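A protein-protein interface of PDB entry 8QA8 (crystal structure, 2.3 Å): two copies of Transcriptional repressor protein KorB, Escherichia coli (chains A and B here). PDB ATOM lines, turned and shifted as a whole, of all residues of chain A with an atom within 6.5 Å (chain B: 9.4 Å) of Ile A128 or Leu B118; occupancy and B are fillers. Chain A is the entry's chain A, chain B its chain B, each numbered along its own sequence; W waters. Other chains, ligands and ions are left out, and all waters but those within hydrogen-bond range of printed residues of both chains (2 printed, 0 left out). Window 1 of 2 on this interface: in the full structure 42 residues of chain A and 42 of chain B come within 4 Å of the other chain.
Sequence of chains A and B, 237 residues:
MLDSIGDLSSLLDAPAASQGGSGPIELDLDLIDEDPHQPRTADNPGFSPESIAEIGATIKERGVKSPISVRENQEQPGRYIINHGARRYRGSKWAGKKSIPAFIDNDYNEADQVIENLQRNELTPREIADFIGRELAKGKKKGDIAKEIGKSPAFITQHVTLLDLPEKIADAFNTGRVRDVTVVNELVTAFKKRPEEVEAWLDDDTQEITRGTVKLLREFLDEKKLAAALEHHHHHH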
ATOM      1  N   GLU A  54       6.280  10.889  23.726  1.00  0.00           N
ATOM      2  CA  GLU A  54       5.959   9.952  22.664  1.00  0.00           C
ATOM      3  C   GLU A  54       7.086   9.879  21.627  1.00  0.00           C
ATOM      4  O   GLU A  54       7.611   8.810  21.339  1.00  0.00           O
ATOM      5  CB  GLU A  54       4.602  10.332  22.086  1.00  0.00           C
ATOM      6  CG  GLU A  54       4.069   9.269  21.164  1.00  0.00           C
ATOM      7  CD  GLU A  54       2.964   9.712  20.247  1.00  0.00           C
ATOM      8  OE1 GLU A  54       1.933  10.151  20.726  1.00  0.00           O
ATOM      9  OE2 GLU A  54       3.152   9.652  19.065  1.00  0.00           O
ATOM     10  N   GLU A 122       0.220  12.186   5.404  1.00  0.00           N
ATOM     11  CA  GLU A 122       0.117  11.083   6.321  1.00  0.00           C
ATOM     12  C   GLU A 122      -0.162   9.772   5.555  1.00  0.00           C
ATOM     13  O   GLU A 122      -0.639   9.751   4.445  1.00  0.00           O
ATOM     14  CB  GLU A 122      -0.963  11.405   7.353  1.00  0.00           C
ATOM     15  CG  GLU A 122      -2.381  11.468   6.779  1.00  0.00           C
ATOM     16  CD  GLU A 122      -3.487  11.884   7.763  1.00  0.00           C
ATOM     17  OE1 GLU A 122      -3.178  12.435   8.883  1.00  0.00           O
ATOM     18  OE2 GLU A 122      -4.676  11.619   7.432  1.00  0.00           O
ATOM     19  N   LEU A 123       0.199   8.655   6.179  1.00  0.00           N
ATOM     20  CA  LEU A 123      -0.348   7.360   5.880  1.00  0.00           C
ATOM     21  C   LEU A 123      -1.836   7.390   6.181  1.00  0.00           C
ATOM     22  O   LEU A 123      -2.257   8.040   7.123  1.00  0.00           O
ATOM     23  CB  LEU A 123       0.381   6.344   6.760  1.00  0.00           C
ATOM     24  CG  LEU A 123       1.875   6.209   6.481  1.00  0.00           C
ATOM     25  CD1 LEU A 123       2.520   5.262   7.473  1.00  0.00           C
ATOM     26  CD2 LEU A 123       2.119   5.772   5.038  1.00  0.00           C
ATOM     27  N   THR A 124      -2.621   6.668   5.373  1.00  0.00           N
ATOM     28  CA  THR A 124      -4.047   6.543   5.634  1.00  0.00           C
ATOM     29  C   THR A 124      -4.257   5.571   6.783  1.00  0.00           C
ATOM     30  O   THR A 124      -3.372   4.795   7.110  1.00  0.00           O
ATOM     31  CB  THR A 124      -4.802   6.032   4.401  1.00  0.00           C
ATOM     32  OG1 THR A 124      -4.245   4.752   4.077  1.00  0.00           O
ATOM     33  CG2 THR A 124      -4.682   6.926   3.187  1.00  0.00           C
ATOM     34  N   PRO A 125      -5.445   5.558   7.417  1.00  0.00           N
ATOM     35  CA  PRO A 125      -5.784   4.521   8.383  1.00  0.00           C
ATOM     36  C   PRO A 125      -5.626   3.097   7.822  1.00  0.00           C
ATOM     37  O   PRO A 125      -5.085   2.209   8.480  1.00  0.00           O
ATOM     38  CB  PRO A 125      -7.255   4.819   8.728  1.00  0.00           C
ATOM     39  CG  PRO A 125      -7.471   6.284   8.382  1.00  0.00           C
ATOM     40  CD  PRO A 125      -6.520   6.554   7.242  1.00  0.00           C
ATOM     41  N   ARG A 126      -6.056   2.895   6.582  1.00  0.00           N
ATOM     42  CA  ARG A 126      -5.968   1.594   5.941  1.00  0.00           C
ATOM     43  C   ARG A 126      -4.500   1.179   5.858  1.00  0.00           C
ATOM     44  O   ARG A 126      -4.162   0.041   6.161  1.00  0.00           O
ATOM     45  CB  ARG A 126      -6.640   1.647   4.558  1.00  0.00           C
ATOM     46  CG  ARG A 126      -6.483   0.410   3.697  1.00  0.00           C
ATOM     47  CD  ARG A 126      -7.682  -0.522   3.816  1.00  0.00           C
ATOM     48  NE  ARG A 126      -7.448  -1.584   4.798  1.00  0.00           N
ATOM     49  CZ  ARG A 126      -8.340  -2.165   5.614  1.00  0.00           C
ATOM     50  NH1 ARG A 126      -9.648  -1.979   5.548  1.00  0.00           N
ATOM     51  NH2 ARG A 126      -7.887  -3.044   6.487  1.00  0.00           N
ATOM     52  N   GLU A 127      -3.620   2.104   5.475  1.00  0.00           N
ATOM     53  CA  GLU A 127      -2.224   1.753   5.305  1.00  0.00           C
ATOM     54  C   GLU A 127      -1.584   1.423   6.648  1.00  0.00           C
ATOM     55  O   GLU A 127      -0.636   0.622   6.695  1.00  0.00           O
ATOM     56  CB  GLU A 127      -1.472   2.895   4.635  1.00  0.00           C
ATOM     57  CG  GLU A 127      -1.777   3.017   3.143  1.00  0.00           C
ATOM     58  CD  GLU A 127      -1.284   4.316   2.528  1.00  0.00           C
ATOM     59  OE1 GLU A 127      -1.051   5.296   3.310  1.00  0.00           O
ATOM     60  OE2 GLU A 127      -0.998   4.294   1.287  1.00  0.00           O
ATOM     61  N   ILE A 128      -2.082   2.046   7.725  1.00  0.00           N
ATOM     62  CA  ILE A 128      -1.521   1.801   9.044  1.00  0.00           C
ATOM     63  C   ILE A 128      -2.028   0.443   9.522  1.00  0.00           C
ATOM     64  O   ILE A 128      -1.248  -0.325  10.067  1.00  0.00           O
ATOM     65  CB  ILE A 128      -1.876   2.948  10.025  1.00  0.00           C
ATOM     66  CG1 ILE A 128      -1.166   4.239   9.636  1.00  0.00           C
ATOM     67  CG2 ILE A 128      -1.567   2.596  11.475  1.00  0.00           C
ATOM     68  CD1 ILE A 128      -1.792   5.491  10.243  1.00  0.00           C
ATOM     69  N   ALA A 129      -3.333   0.193   9.365  1.00  0.00           N
ATOM     70  CA  ALA A 129      -3.918  -1.095   9.682  1.00  0.00           C
ATOM     71  C   ALA A 129      -3.170  -2.218   8.955  1.00  0.00           C
ATOM     72  O   ALA A 129      -2.810  -3.221   9.566  1.00  0.00           O
ATOM     73  CB  ALA A 129      -5.388  -1.113   9.332  1.00  0.00           C
ATOM     74  N   ASP A 130      -2.925  -2.046   7.661  1.00  0.00           N
ATOM     75  CA  ASP A 130      -2.322  -3.108   6.858  1.00  0.00           C
ATOM     76  C   ASP A 130      -0.887  -3.353   7.313  1.00  0.00           C
ATOM     77  O   ASP A 130      -0.442  -4.500   7.318  1.00  0.00           O
ATOM     78  CB  ASP A 130      -2.384  -2.825   5.362  1.00  0.00           C
ATOM     79  CG  ASP A 130      -3.788  -2.965   4.791  1.00  0.00           C
ATOM     80  OD1 ASP A 130      -4.700  -3.425   5.520  1.00  0.00           O
ATOM     81  OD2 ASP A 130      -3.966  -2.585   3.614  1.00  0.00           O
ATOM     82  N   PHE A 131      -0.171  -2.304   7.732  1.00  0.00           N
ATOM     83  CA  PHE A 131       1.143  -2.536   8.301  1.00  0.00           C
ATOM     84  C   PHE A 131       1.028  -3.397   9.562  1.00  0.00           C
ATOM     85  O   PHE A 131       1.785  -4.354   9.742  1.00  0.00           O
ATOM     86  CB  PHE A 131       1.827  -1.222   8.657  1.00  0.00           C
ATOM     87  CG  PHE A 131       3.076  -1.433   9.458  1.00  0.00           C
ATOM     88  CD1 PHE A 131       4.241  -1.834   8.838  1.00  0.00           C
ATOM     89  CD2 PHE A 131       3.059  -1.287  10.826  1.00  0.00           C
ATOM     90  CE1 PHE A 131       5.384  -2.070   9.566  1.00  0.00           C
ATOM     91  CE2 PHE A 131       4.202  -1.514  11.561  1.00  0.00           C
ATOM     92  CZ  PHE A 131       5.361  -1.896  10.934  1.00  0.00           C
ATOM     93  N   ILE A 132       0.054  -3.059  10.413  1.00  0.00           N
ATOM     94  CA  ILE A 132      -0.133  -3.777  11.654  1.00  0.00           C
ATOM     95  C   ILE A 132      -0.459  -5.233  11.302  1.00  0.00           C
ATOM     96  O   ILE A 132       0.135  -6.162  11.831  1.00  0.00           O
ATOM     97  CB  ILE A 132      -1.197  -3.074  12.521  1.00  0.00           C
ATOM     98  CG1 ILE A 132      -0.705  -1.712  13.025  1.00  0.00           C
ATOM     99  CG2 ILE A 132      -1.616  -3.949  13.696  1.00  0.00           C
ATOM    100  CD1 ILE A 132      -1.805  -0.813  13.532  1.00  0.00           C
ATOM    101  N   GLY A 133      -1.378  -5.409  10.358  1.00  0.00           N
ATOM    102  CA  GLY A 133      -1.749  -6.720   9.814  1.00  0.00           C
ATOM    103  C   GLY A 133      -0.554  -7.567   9.396  1.00  0.00           C
ATOM    104  O   GLY A 133      -0.508  -8.740   9.717  1.00  0.00           O
ATOM    105  N   ILE A 149       6.400   1.328  16.771  1.00  0.00           N
ATOM    106  CA  ILE A 149       5.993   2.552  16.088  1.00  0.00           C
ATOM    107  C   ILE A 149       5.714   3.686  17.084  1.00  0.00           C
ATOM    108  O   ILE A 149       5.221   4.735  16.707  1.00  0.00           O
ATOM    109  CB  ILE A 149       4.781   2.328  15.162  1.00  0.00           C
ATOM    110  CG1 ILE A 149       3.486   2.019  15.915  1.00  0.00           C
ATOM    111  CG2 ILE A 149       5.097   1.248  14.137  1.00  0.00           C
ATOM    112  CD1 ILE A 149       2.274   1.948  15.019  1.00  0.00           C
ATOM    113  N   LYS A 151       3.491   4.073  19.468  1.00  0.00           N
ATOM    114  CA  LYS A 151       2.109   4.420  19.723  1.00  0.00           C
ATOM    115  C   LYS A 151       1.563   3.586  20.864  1.00  0.00           C
ATOM    116  O   LYS A 151       2.204   2.653  21.317  1.00  0.00           O
ATOM    117  CB  LYS A 151       1.321   4.224  18.431  1.00  0.00           C
ATOM    118  CG  LYS A 151       1.702   5.201  17.335  1.00  0.00           C
ATOM    119  CD  LYS A 151       0.807   6.382  17.543  1.00  0.00           C
ATOM    120  CE  LYS A 151       1.226   7.656  16.879  1.00  0.00           C
ATOM    121  NZ  LYS A 151       0.325   8.745  17.347  1.00  0.00           N
ATOM    122  N   PHE A 155      -4.196   2.728  20.181  1.00  0.00           N
ATOM    123  CA  PHE A 155      -4.075   3.146  18.791  1.00  0.00           C
ATOM    124  C   PHE A 155      -4.033   1.908  17.881  1.00  0.00           C
ATOM    125  O   PHE A 155      -4.638   1.904  16.810  1.00  0.00           O
ATOM    126  CB  PHE A 155      -2.839   4.036  18.630  1.00  0.00           C
ATOM    127  CG  PHE A 155      -2.526   4.500  17.226  1.00  0.00           C
ATOM    128  CD1 PHE A 155      -2.931   5.759  16.783  1.00  0.00           C
ATOM    129  CD2 PHE A 155      -1.745   3.713  16.372  1.00  0.00           C
ATOM    130  CE1 PHE A 155      -2.612   6.206  15.506  1.00  0.00           C
ATOM    131  CE2 PHE A 155      -1.395   4.181  15.110  1.00  0.00           C
ATOM    132  CZ  PHE A 155      -1.834   5.425  14.680  1.00  0.00           C
ATOM    133  N   ILE A 156      -3.289   0.876  18.312  1.00  0.00           N
ATOM    134  CA  ILE A 156      -3.212  -0.379  17.595  1.00  0.00           C
ATOM    135  C   ILE A 156      -4.605  -0.989  17.513  1.00  0.00           C
ATOM    136  O   ILE A 156      -5.060  -1.319  16.449  1.00  0.00           O
ATOM    137  CB  ILE A 156      -2.226  -1.341  18.274  1.00  0.00           C
ATOM    138  CG1 ILE A 156      -0.823  -0.762  18.373  1.00  0.00           C
ATOM    139  CG2 ILE A 156      -2.198  -2.670  17.536  1.00  0.00           C
ATOM    140  CD1 ILE A 156      -0.255  -0.268  17.072  1.00  0.00           C
ATOM    141  N   HIS A 159      -6.953   0.579  14.935  1.00  0.00           N
ATOM    142  CA  HIS A 159      -6.600   0.291  13.562  1.00  0.00           C
ATOM    143  C   HIS A 159      -6.866  -1.191  13.208  1.00  0.00           C
ATOM    144  O   HIS A 159      -7.345  -1.510  12.111  1.00  0.00           O
ATOM    145  CB  HIS A 159      -5.175   0.775  13.284  1.00  0.00           C
ATOM    146  CG  HIS A 159      -5.102   2.265  13.195  1.00  0.00           C
ATOM    147  ND1 HIS A 159      -5.055   3.095  14.300  1.00  0.00           N
ATOM    148  CD2 HIS A 159      -5.084   3.082  12.128  1.00  0.00           C
ATOM    149  CE1 HIS A 159      -5.000   4.356  13.894  1.00  0.00           C
ATOM    150  NE2 HIS A 159      -5.024   4.367  12.581  1.00  0.00           N
ATOM    151  N   PRO B  39       5.489   1.719   3.514  1.00  0.00           N
ATOM    152  CA  PRO B  39       4.090   1.654   3.958  1.00  0.00           C
ATOM    153  C   PRO B  39       3.117   2.569   3.208  1.00  0.00           C
ATOM    154  O   PRO B  39       1.919   2.353   3.281  1.00  0.00           O
ATOM    155  CB  PRO B  39       4.211   2.045   5.439  1.00  0.00           C
ATOM    156  CG  PRO B  39       5.414   2.962   5.473  1.00  0.00           C
ATOM    157  CD  PRO B  39       6.388   2.383   4.459  1.00  0.00           C
ATOM    158  N   ARG B  40       3.614   3.592   2.515  1.00  0.00           N
ATOM    159  CA  ARG B  40       2.755   4.392   1.649  1.00  0.00           C
ATOM    160  C   ARG B  40       2.468   3.677   0.325  1.00  0.00           C
ATOM    161  O   ARG B  40       3.393   3.360  -0.420  1.00  0.00           O
ATOM    162  CB  ARG B  40       3.392   5.737   1.325  1.00  0.00           C
ATOM    163  CG  ARG B  40       2.366   6.763   0.863  1.00  0.00           C
ATOM    164  CD  ARG B  40       2.950   8.045   0.340  1.00  0.00           C
ATOM    165  NE  ARG B  40       3.817   8.728   1.266  1.00  0.00           N
ATOM    166  CZ  ARG B  40       3.403   9.569   2.206  1.00  0.00           C
ATOM    167  NH1 ARG B  40       2.119   9.864   2.333  1.00  0.00           N
ATOM    168  NH2 ARG B  40       4.295  10.116   3.005  1.00  0.00           N
ATOM    169  N   THR B  41       1.185   3.399   0.046  1.00  0.00           N
ATOM    170  CA  THR B  41       0.808   2.688  -1.160  1.00  0.00           C
ATOM    171  C   THR B  41       0.455   3.666  -2.274  1.00  0.00           C
ATOM    172  O   THR B  41       0.358   4.870  -2.066  1.00  0.00           O
ATOM    173  CB  THR B  41      -0.377   1.757  -0.904  1.00  0.00           C
ATOM    174  OG1 THR B  41      -1.506   2.570  -0.608  1.00  0.00           O
ATOM    175  CG2 THR B  41      -0.079   0.757   0.207  1.00  0.00           C
ATOM    176  N   ASN B  44      -2.221   6.396  -2.040  1.00  0.00           N
ATOM    177  CA  ASN B  44      -2.106   7.430  -1.027  1.00  0.00           C
ATOM    178  C   ASN B  44      -2.220   8.830  -1.645  1.00  0.00           C
ATOM    179  O   ASN B  44      -1.468   9.171  -2.554  1.00  0.00           O
ATOM    180  CB  ASN B  44      -0.802   7.274  -0.239  1.00  0.00           C
ATOM    181  CG  ASN B  44      -0.631   8.287   0.886  1.00  0.00           C
ATOM    182  OD1 ASN B  44      -0.127   9.387   0.683  1.00  0.00           O
ATOM    183  ND2 ASN B  44      -0.961   7.875   2.096  1.00  0.00           N
ATOM    184  N   TYR B 108      18.160   0.476   9.313  1.00  0.00           N
ATOM    185  CA  TYR B 108      16.853   1.091   9.206  1.00  0.00           C
ATOM    186  C   TYR B 108      15.856  -0.007   8.864  1.00  0.00           C
ATOM    187  O   TYR B 108      16.087  -0.720   7.902  1.00  0.00           O
ATOM    188  CB  TYR B 108      16.902   2.156   8.099  1.00  0.00           C
ATOM    189  CG  TYR B 108      15.799   3.195   8.117  1.00  0.00           C
ATOM    190  CD1 TYR B 108      16.077   4.508   8.451  1.00  0.00           C
ATOM    191  CD2 TYR B 108      14.485   2.888   7.793  1.00  0.00           C
ATOM    192  CE1 TYR B 108      15.094   5.485   8.473  1.00  0.00           C
ATOM    193  CE2 TYR B 108      13.483   3.852   7.828  1.00  0.00           C
ATOM    194  CZ  TYR B 108      13.789   5.149   8.188  1.00  0.00           C
ATOM    195  OH  TYR B 108      12.855   6.144   8.270  1.00  0.00           O
ATOM    196  N   ALA B 111       9.554  -0.782  10.530  1.00  0.00           N
ATOM    197  CA  ALA B 111       8.933  -0.002  11.598  1.00  0.00           C
ATOM    198  C   ALA B 111       9.408   1.462  11.618  1.00  0.00           C
ATOM    199  O   ALA B 111       8.604   2.358  11.834  1.00  0.00           O
ATOM    200  CB  ALA B 111       9.193  -0.673  12.916  1.00  0.00           C
ATOM    201  N   ASP B 112      10.705   1.689  11.367  1.00  0.00           N
ATOM    202  CA  ASP B 112      11.262   3.026  11.313  1.00  0.00           C
ATOM    203  C   ASP B 112      10.531   3.827  10.254  1.00  0.00           C
ATOM    204  O   ASP B 112      10.291   5.011  10.450  1.00  0.00           O
ATOM    205  CB  ASP B 112      12.774   3.009  11.071  1.00  0.00           C
ATOM    206  CG  ASP B 112      13.599   2.387  12.200  1.00  0.00           C
ATOM    207  OD1 ASP B 112      13.123   2.379  13.375  1.00  0.00           O
ATOM    208  OD2 ASP B 112      14.704   1.856  11.910  1.00  0.00           O
ATOM    209  N   GLN B 113      10.138   3.190   9.142  1.00  0.00           N
ATOM    210  CA  GLN B 113       9.466   3.888   8.048  1.00  0.00           C
ATOM    211  C   GLN B 113       8.104   4.367   8.522  1.00  0.00           C
ATOM    212  O   GLN B 113       7.672   5.420   8.075  1.00  0.00           O
ATOM    213  CB  GLN B 113       9.258   3.004   6.804  1.00  0.00           C
ATOM    214  CG  GLN B 113      10.544   2.514   6.153  1.00  0.00           C
ATOM    215  CD  GLN B 113      10.358   1.540   4.999  1.00  0.00           C
ATOM    216  OE1 GLN B 113       9.599   0.565   5.053  1.00  0.00           O
ATOM    217  NE2 GLN B 113      11.127   1.765   3.947  1.00  0.00           N
ATOM    218  N   VAL B 114       7.430   3.609   9.389  1.00  0.00           N
ATOM    219  CA  VAL B 114       6.143   4.062   9.895  1.00  0.00           C
ATOM    220  C   VAL B 114       6.357   5.169  10.934  1.00  0.00           C
ATOM    221  O   VAL B 114       5.617   6.145  10.949  1.00  0.00           O
ATOM    222  CB  VAL B 114       5.334   2.891  10.458  1.00  0.00           C
ATOM    223  CG1 VAL B 114       4.022   3.318  11.069  1.00  0.00           C
ATOM    224  CG2 VAL B 114       5.103   1.833   9.376  1.00  0.00           C
ATOM    225  N   ILE B 115       7.402   5.049  11.768  1.00  0.00           N
ATOM    226  CA  ILE B 115       7.784   6.098  12.707  1.00  0.00           C
ATOM    227  C   ILE B 115       7.990   7.442  11.992  1.00  0.00           C
ATOM    228  O   ILE B 115       7.434   8.424  12.416  1.00  0.00           O
ATOM    229  CB  ILE B 115       9.043   5.667  13.488  1.00  0.00           C
ATOM    230  CG1 ILE B 115       8.728   4.622  14.550  1.00  0.00           C
ATOM    231  CG2 ILE B 115       9.756   6.878  14.079  1.00  0.00           C
ATOM    232  CD1 ILE B 115       9.970   4.130  15.256  1.00  0.00           C
ATOM    233  N   GLU B 116       8.767   7.476  10.896  1.00  0.00           N
ATOM    234  CA  GLU B 116       9.113   8.700  10.200  1.00  0.00           C
ATOM    235  C   GLU B 116       7.844   9.500   9.904  1.00  0.00           C
ATOM    236  O   GLU B 116       7.836  10.730   9.882  1.00  0.00           O
ATOM    237  CB  GLU B 116       9.836   8.390   8.889  1.00  0.00           C
ATOM    238  CG  GLU B 116      10.175   9.608   7.986  1.00  0.00           C
ATOM    239  CD  GLU B 116       9.267  10.066   6.840  1.00  0.00           C
ATOM    240  OE1 GLU B 116       8.472   9.281   6.232  1.00  0.00           O
ATOM    241  OE2 GLU B 116       9.344  11.280   6.547  1.00  0.00           O
ATOM    242  N   ASN B 117       6.743   8.782   9.737  1.00  0.00           N
ATOM    243  CA  ASN B 117       5.525   9.361   9.242  1.00  0.00           C
ATOM    244  C   ASN B 117       4.546   9.655  10.376  1.00  0.00           C
ATOM    245  O   ASN B 117       3.818  10.650  10.297  1.00  0.00           O
ATOM    246  CB  ASN B 117       4.951   8.382   8.234  1.00  0.00           C
ATOM    247  CG  ASN B 117       3.819   8.982   7.463  1.00  0.00           C
ATOM    248  OD1 ASN B 117       2.693   9.053   7.985  1.00  0.00           O
ATOM    249  ND2 ASN B 117       4.146   9.449   6.258  1.00  0.00           N
ATOM    250  N   LEU B 118       4.468   8.788  11.396  1.00  0.00           N
ATOM    251  CA  LEU B 118       3.472   8.952  12.429  1.00  0.00           C
ATOM    252  C   LEU B 118       3.978   9.893  13.540  1.00  0.00           C
ATOM    253  O   LEU B 118       3.175  10.424  14.307  1.00  0.00           O
ATOM    254  CB  LEU B 118       3.141   7.592  13.037  1.00  0.00           C
ATOM    255  CG  LEU B 118       2.323   6.610  12.194  1.00  0.00           C
ATOM    256  CD1 LEU B 118       1.817   5.461  13.047  1.00  0.00           C
ATOM    257  CD2 LEU B 118       1.147   7.296  11.535  1.00  0.00           C
ATOM    258  N   GLN B 119       5.298   9.995  13.728  1.00  0.00           N
ATOM    259  CA  GLN B 119       5.876  10.716  14.858  1.00  0.00           C
ATOM    260  C   GLN B 119       6.145  12.161  14.432  1.00  0.00           C
ATOM    261  O   GLN B 119       7.306  12.577  14.328  1.00  0.00           O
ATOM    262  CB  GLN B 119       7.154  10.036  15.353  1.00  0.00           C
ATOM    263  CG  GLN B 119       6.883   8.699  16.025  1.00  0.00           C
ATOM    264  CD  GLN B 119       6.005   8.780  17.228  1.00  0.00           C
ATOM    265  OE1 GLN B 119       6.030   9.780  17.954  1.00  0.00           O
ATOM    266  NE2 GLN B 119       5.307   7.689  17.504  1.00  0.00           N
ATOM    267  N   ARG B 120       5.059  12.897  14.147  1.00  0.00           N
ATOM    268  CA  ARG B 120       5.172  14.289  13.762  1.00  0.00           C
ATOM    269  C   ARG B 120       3.820  14.961  13.980  1.00  0.00           C
ATOM    270  O   ARG B 120       2.785  14.302  14.030  1.00  0.00           O
ATOM    271  CB  ARG B 120       5.673  14.473  12.331  1.00  0.00           C
ATOM    272  CG  ARG B 120       4.887  13.703  11.275  1.00  0.00           C
ATOM    273  CD  ARG B 120       5.014  14.271   9.886  1.00  0.00           C
ATOM    274  NE  ARG B 120       4.969  13.364   8.751  1.00  0.00           N
ATOM    275  CZ  ARG B 120       3.970  13.273   7.885  1.00  0.00           C
ATOM    276  NH1 ARG B 120       2.710  13.546   8.204  1.00  0.00           N
ATOM    277  NH2 ARG B 120       4.269  12.854   6.681  1.00  0.00           N
ATOM    278  N   ASN B 121       3.878  16.279  14.198  1.00  0.00           N
ATOM    279  CA  ASN B 121       2.736  17.058  14.631  1.00  0.00           C
ATOM    280  C   ASN B 121       2.641  18.335  13.798  1.00  0.00           C
ATOM    281  O   ASN B 121       3.652  18.944  13.487  1.00  0.00           O
ATOM    282  CB  ASN B 121       2.877  17.453  16.089  1.00  0.00           C
ATOM    283  CG  ASN B 121       2.676  16.279  17.018  1.00  0.00           C
ATOM    284  OD1 ASN B 121       3.578  15.470  17.243  1.00  0.00           O
ATOM    285  ND2 ASN B 121       1.499  16.195  17.609  1.00  0.00           N
ATOM    286  N   GLU B 122       1.426  18.715  13.453  1.00  0.00           N
ATOM    287  CA  GLU B 122       1.202  19.879  12.603  1.00  0.00           C
ATOM    288  C   GLU B 122       1.260  21.182  13.428  1.00  0.00           C
ATOM    289  O   GLU B 122       1.048  21.196  14.624  1.00  0.00           O
ATOM    290  CB  GLU B 122      -0.142  19.693  11.879  1.00  0.00           C
ATOM    291  CG  GLU B 122      -1.352  19.745  12.816  1.00  0.00           C
ATOM    292  CD  GLU B 122      -2.662  19.124  12.339  1.00  0.00           C
ATOM    293  OE1 GLU B 122      -2.799  18.840  11.097  1.00  0.00           O
ATOM    294  OE2 GLU B 122      -3.536  18.902  13.236  1.00  0.00           O
HETATM  295  O   HOH W   1       1.165   0.406   4.735  1.00  0.00           O
HETATM  296  O   HOH W   2       0.463   9.789  14.906  1.00  0.00           O
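OE2 of Glu A54 is in salt-bridge range of NZ of Lys A151, 3.4 Å away.
A ring nitrogen (ND1) of His A159 is in hydrogen-bond range of the backbone carbonyl oxygen (O) of Phe A155 (2.8 Å).
The backbone NH of Thr A124 lies within hydrogen-bond range of the side-chain carboxylate of Glu A127, 2.9 Å away.
The backbone carbonyl oxygen (O) of Asn B117 is in hydrogen-bond range of the guanidinium group (NE) of Arg B120, at 3.3 Å.
The guanidinium group of Arg B40 is in hydrogen-bond range of the side-chain amide oxygen of Asn B44, at 2.8 Å.
The guanidinium group (NH2) of Arg B40 lies close to the side-chain amide nitrogen (ND2) of Asn B117 (3.3 Å).
Position printed for both chains: 122.
The side-chain carboxylate (OE1) of Glu A127 sits at hydrogen-bond distance from the side-chain amide nitrogen (ND2) of Asn B44 (2.9 Å).
The backbone carbonyl oxygen (O) of Glu A122 is in hydrogen-bond range of the side-chain amide nitrogen (ND2) of Asn B44 (3.0 Å).
NE2 of Gln B119 sits at hydrogen-bond distance from O of Ile A149 (3.1 Å).
The side-chain carboxylate (OE2) of Glu A127 sits at hydrogen-bond distance from the side-chain hydroxyl (OG1) of Thr B41.
OE1 of Gln B119 sits close to OE2 of Glu A54 (3.1 Å).
NH1 of Arg B40 is in hydrogen-bond range of O of Glu A122 (3.5 Å).
The backbone NH of Leu A123 lies within hydrogen-bond range of the side-chain amide oxygen of Asn B117 (3.1 Å).
Glu A122 touches Asn B117 (CA to OD1, 3.7 Å).
CD2 of Leu A123 touches C of Pro B39, at 3.8 Å.
Arg B40 touches Leu A123.
Thr A124 touches Asn B44 (N to ND2, 3.9 Å).
C of Arg B40 touches OE2 of Glu A127, at 3.6 Å.
CD2 of Leu B118 touches CD1 of Ile A128, 3.7 Å away.
CG2 of Val B114 touches CD1 of Phe A131, at 3.8 Å.
Ile A149 touches Val B114.
Ile A149 touches Ile B115.
Leu B118 touches Phe A155 (CD1 to CZ, 3.9997 Å).
Water W1 lies within hydrogen-bond range of the backbone carbonyl oxygen (O) of Pro B39 (2.5 Å) and the backbone carbonyl oxygen (O) of Glu A127 (2.7 Å).
Water W2 bridges NZ of Lys A151 (2.7 Å) and O of Leu B118 (2.8 Å).
Ile A128 touches just one residue of chain B: Leu B118.
Of the printed residues of chain A, Leu B118 touches Ile A128 (3.7 Å) and Phe A155 (3.9997 Å).
Printed residues of chain B within 4 Å of Phe A155: Leu B118.
Of the printed residues of chain B, Leu A123 touches Pro B39, Arg B40, Asn B44 and Asn B117.
Printed residues of chain B within 4 Å of Ile A149: Val B114, Ile B115 and Gln B119.
Printed residues of chain A within 4 Å of Arg B120: Glu A122 (3.99 Å).
Asp A130 touches none of the printed residues of chain B.
Asp B112 touches none of the printed residues of chain A.
Printed residues of chain B that touch a printed residue of chain A: Pro B39, Arg B40, Thr B41, Asn B44, Val B114, Ile B115, Asn B117, Leu B118, Gln B119 and Arg B120.
Hydrophobic or aromatic side chains of chain B that line the printed part of chain A: Val B114, Ile B115 and Leu B118.
Hydrophobic or aromatic side chains of chain A within 4 Å of the printed part of chain B: Leu A123, Ile A128, Phe A131, Ile A149 and Phe A155.
Among the printed residues, 20 pairs touch across the chains.
Among the printed residues, no Asp or Glu carboxylate lies within 4 Å of a Lys or Arg side-chain nitrogen of the other chain.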
